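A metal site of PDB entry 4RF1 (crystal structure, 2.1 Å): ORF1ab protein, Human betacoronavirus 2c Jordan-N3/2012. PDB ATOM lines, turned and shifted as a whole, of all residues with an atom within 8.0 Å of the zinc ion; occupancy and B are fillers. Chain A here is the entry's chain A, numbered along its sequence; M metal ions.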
ATOM      1  N   TRP A 192     -28.841  13.666   8.690  1.00  0.00           N
ATOM      2  CA  TRP A 192     -28.620  13.875  10.109  1.00  0.00           C
ATOM      3  C   TRP A 192     -28.356  12.572  10.866  1.00  0.00           C
ATOM      4  O   TRP A 192     -28.863  11.512  10.520  1.00  0.00           O
ATOM      5  CB  TRP A 192     -29.802  14.617  10.748  1.00  0.00           C
ATOM      6  CG  TRP A 192     -31.095  13.854  10.781  1.00  0.00           C
ATOM      7  CD1 TRP A 192     -31.598  13.144  11.836  1.00  0.00           C
ATOM      8  CD2 TRP A 192     -32.062  13.749   9.727  1.00  0.00           C
ATOM      9  NE1 TRP A 192     -32.811  12.594  11.498  1.00  0.00           N
ATOM     10  CE2 TRP A 192     -33.114  12.951  10.207  1.00  0.00           C
ATOM     11  CE3 TRP A 192     -32.129  14.245   8.423  1.00  0.00           C
ATOM     12  CZ2 TRP A 192     -34.229  12.639   9.437  1.00  0.00           C
ATOM     13  CZ3 TRP A 192     -33.243  13.933   7.653  1.00  0.00           C
ATOM     14  CH2 TRP A 192     -34.269  13.139   8.165  1.00  0.00           C
ATOM     15  N   CYS A 193     -27.520  12.695  11.898  1.00  0.00           N
ATOM     16  CA  CYS A 193     -27.145  11.599  12.767  1.00  0.00           C
ATOM     17  C   CYS A 193     -26.935  12.150  14.172  1.00  0.00           C
ATOM     18  O   CYS A 193     -26.331  13.204  14.341  1.00  0.00           O
ATOM     19  CB  CYS A 193     -25.871  10.910  12.248  1.00  0.00           C
ATOM     20  SG  CYS A 193     -25.086   9.773  13.400  1.00  0.00           S
ATOM     21  N   ASN A 194     -27.442  11.433  15.176  1.00  0.00           N
ATOM     22  CA  ASN A 194     -27.418  11.920  16.552  1.00  0.00           C
ATOM     23  C   ASN A 194     -26.019  12.200  17.103  1.00  0.00           C
ATOM     24  O   ASN A 194     -25.853  13.023  17.998  1.00  0.00           O
ATOM     25  CB  ASN A 194     -28.135  10.938  17.466  1.00  0.00           C
ATOM     26  CG  ASN A 194     -29.644  10.941  17.263  1.00  0.00           C
ATOM     27  OD1 ASN A 194     -30.144  11.485  16.285  1.00  0.00           O
ATOM     28  ND2 ASN A 194     -30.363  10.336  18.203  1.00  0.00           N
ATOM     29  N   VAL A 195     -25.020  11.513  16.566  1.00  0.00           N
ATOM     30  CA  VAL A 195     -23.649  11.674  17.035  1.00  0.00           C
ATOM     31  C   VAL A 195     -22.853  12.650  16.176  1.00  0.00           C
ATOM     32  O   VAL A 195     -22.180  13.551  16.687  1.00  0.00           O
ATOM     33  CB  VAL A 195     -22.903  10.325  17.073  1.00  0.00           C
ATOM     34  CG1 VAL A 195     -21.437  10.518  17.438  1.00  0.00           C
ATOM     35  CG2 VAL A 195     -23.582   9.369  18.056  1.00  0.00           C
ATOM     36  N   CYS A 196     -22.952  12.485  14.860  1.00  0.00           N
ATOM     37  CA  CYS A 196     -22.175  13.304  13.928  1.00  0.00           C
ATOM     38  C   CYS A 196     -22.793  14.692  13.720  1.00  0.00           C
ATOM     39  O   CYS A 196     -22.082  15.679  13.589  1.00  0.00           O
ATOM     40  CB  CYS A 196     -22.027  12.588  12.588  1.00  0.00           C
ATOM     41  SG  CYS A 196     -21.006  11.096  12.675  1.00  0.00           S
ATOM     42  N   GLY A 197     -24.126  14.749  13.698  1.00  0.00           N
ATOM     43  CA  GLY A 197     -24.813  16.019  13.553  1.00  0.00           C
ATOM     44  C   GLY A 197     -25.599  16.140  12.257  1.00  0.00           C
ATOM     45  O   GLY A 197     -25.784  15.168  11.529  1.00  0.00           O
ATOM     46  N   VAL A 227     -26.859   3.426   7.467  1.00  0.00           N
ATOM     47  CA  VAL A 227     -25.852   3.428   8.535  1.00  0.00           C
ATOM     48  C   VAL A 227     -24.799   4.508   8.313  1.00  0.00           C
ATOM     49  O   VAL A 227     -24.238   4.637   7.219  1.00  0.00           O
ATOM     50  CB  VAL A 227     -25.150   2.053   8.639  1.00  0.00           C
ATOM     51  CG1 VAL A 227     -24.102   2.081   9.731  1.00  0.00           C
ATOM     52  CG2 VAL A 227     -26.168   0.954   8.898  1.00  0.00           C
ATOM     53  N   CYS A 228     -24.538   5.300   9.350  1.00  0.00           N
ATOM     54  CA  CYS A 228     -23.549   6.363   9.283  1.00  0.00           C
ATOM     55  C   CYS A 228     -22.124   5.814   9.325  1.00  0.00           C
ATOM     56  O   CYS A 228     -21.915   4.647   9.670  1.00  0.00           O
ATOM     57  CB  CYS A 228     -23.747   7.373  10.427  1.00  0.00           C
ATOM     58  SG  CYS A 228     -22.604   8.777  10.431  1.00  0.00           S
ATOM     59  N   GLN A 229     -21.165   6.659   8.973  1.00  0.00           N
ATOM     60  CA  GLN A 229     -19.758   6.300   9.012  1.00  0.00           C
ATOM     61  C   GLN A 229     -19.329   5.882  10.419  1.00  0.00           C
ATOM     62  O   GLN A 229     -18.471   5.012  10.587  1.00  0.00           O
ATOM     63  CB  GLN A 229     -18.895   7.461   8.516  1.00  0.00           C
ATOM     64  CG  GLN A 229     -17.404   7.211   8.595  1.00  0.00           C
ATOM     65  CD  GLN A 229     -16.956   6.047   7.735  1.00  0.00           C
ATOM     66  OE1 GLN A 229     -17.239   5.990   6.544  1.00  0.00           O
ATOM     67  NE2 GLN A 229     -16.246   5.101   8.345  1.00  0.00           N
ATOM     68  N   CYS A 230     -19.939   6.503  11.425  1.00  0.00           N
ATOM     69  CA  CYS A 230     -19.634   6.189  12.814  1.00  0.00           C
ATOM     70  C   CYS A 230     -20.266   4.865  13.245  1.00  0.00           C
ATOM     71  O   CYS A 230     -19.954   4.331  14.315  1.00  0.00           O
ATOM     72  CB  CYS A 230     -20.114   7.308  13.736  1.00  0.00           C
ATOM     73  SG  CYS A 230     -21.904   7.461  13.860  1.00  0.00           S
ATOM     74  N   GLY A 231     -21.155   4.329  12.404  1.00  0.00           N
ATOM     75  CA  GLY A 231     -21.787   3.053  12.674  1.00  0.00           C
ATOM     76  C   GLY A 231     -23.190   3.171  13.223  1.00  0.00           C
ATOM     77  O   GLY A 231     -23.857   2.167  13.463  1.00  0.00           O
ATOM     78  N   GLY A 232     -23.657   4.407  13.416  1.00  0.00           N
ATOM     79  CA  GLY A 232     -24.984   4.640  13.960  1.00  0.00           C
ATOM     80  C   GLY A 232     -26.037   4.857  12.893  1.00  0.00           C
ATOM     81  O   GLY A 232     -25.738   4.825  11.703  1.00  0.00           O
ATOM     82  N   GLU A 233     -27.274   5.077  13.323  1.00  0.00           N
ATOM     83  CA  GLU A 233     -28.383   5.288  12.406  1.00  0.00           C
ATOM     84  C   GLU A 233     -28.320   6.670  11.765  1.00  0.00           C
ATOM     85  O   GLU A 233     -28.307   7.689  12.447  1.00  0.00           O
ATOM     86  CB  GLU A 233     -29.717   5.122  13.138  1.00  0.00           C
ATOM     87  CG  GLU A 233     -30.940   5.182  12.234  1.00  0.00           C
ATOM     88  CD  GLU A 233     -32.239   5.034  13.007  1.00  0.00           C
ATOM     89  OE1 GLU A 233     -32.286   5.442  14.178  1.00  0.00           O
ATOM     90  OE2 GLU A 233     -33.211   4.492  12.432  1.00  0.00           O
ATOM     91  N   ARG A 234     -28.272   6.688  10.437  1.00  0.00           N
ATOM     92  CA  ARG A 234     -28.233   7.940   9.686  1.00  0.00           C
ATOM     93  C   ARG A 234     -29.440   8.060   8.778  1.00  0.00           C
ATOM     94  O   ARG A 234     -29.908   7.067   8.224  1.00  0.00           O
ATOM     95  CB  ARG A 234     -26.941   8.040   8.867  1.00  0.00           C
ATOM     96  CG  ARG A 234     -26.717   9.391   8.217  1.00  0.00           C
ATOM     97  CD  ARG A 234     -25.297   9.515   7.676  1.00  0.00           C
ATOM     98  NE  ARG A 234     -25.034  10.857   7.148  1.00  0.00           N
ATOM     99  CZ  ARG A 234     -24.538  11.863   7.864  1.00  0.00           C
ATOM    100  NH1 ARG A 234     -24.257  11.688   9.147  1.00  0.00           N
ATOM    101  NH2 ARG A 234     -24.329  13.034   7.301  1.00  0.00           N
HETATM  102 ZN    ZN M   1     -22.811   9.406  12.713  1.00  0.00          ZN
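The side-chain sulfur (SG) of Cys 228 sits close to the guanidinium group (NH1) of Arg 234, at 3.6 Å.
The side-chain sulfur (SG) of Cys 193 sits close to the backbone NH (N) of Val 195, 3.6 Å away.
The backbone NH of Gly 232 lies close to the side-chain sulfur of Cys 230 (3.5 Å).
Within 4 Å of the zinc ion: Cys 193, Cys 196, Cys 228 and Cys 230.
The nearest printed residue that does not touch the zinc ion is Val 195 (4.5 Å).
The zinc ion is bound by the side-chain sulfur of Cys 228, the side-chain sulfur of Cys 193, the side-chain sulfur of Cys 230 and the side-chain sulfur of Cys 196.
The zinc ion has four donor atoms within binding distance.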
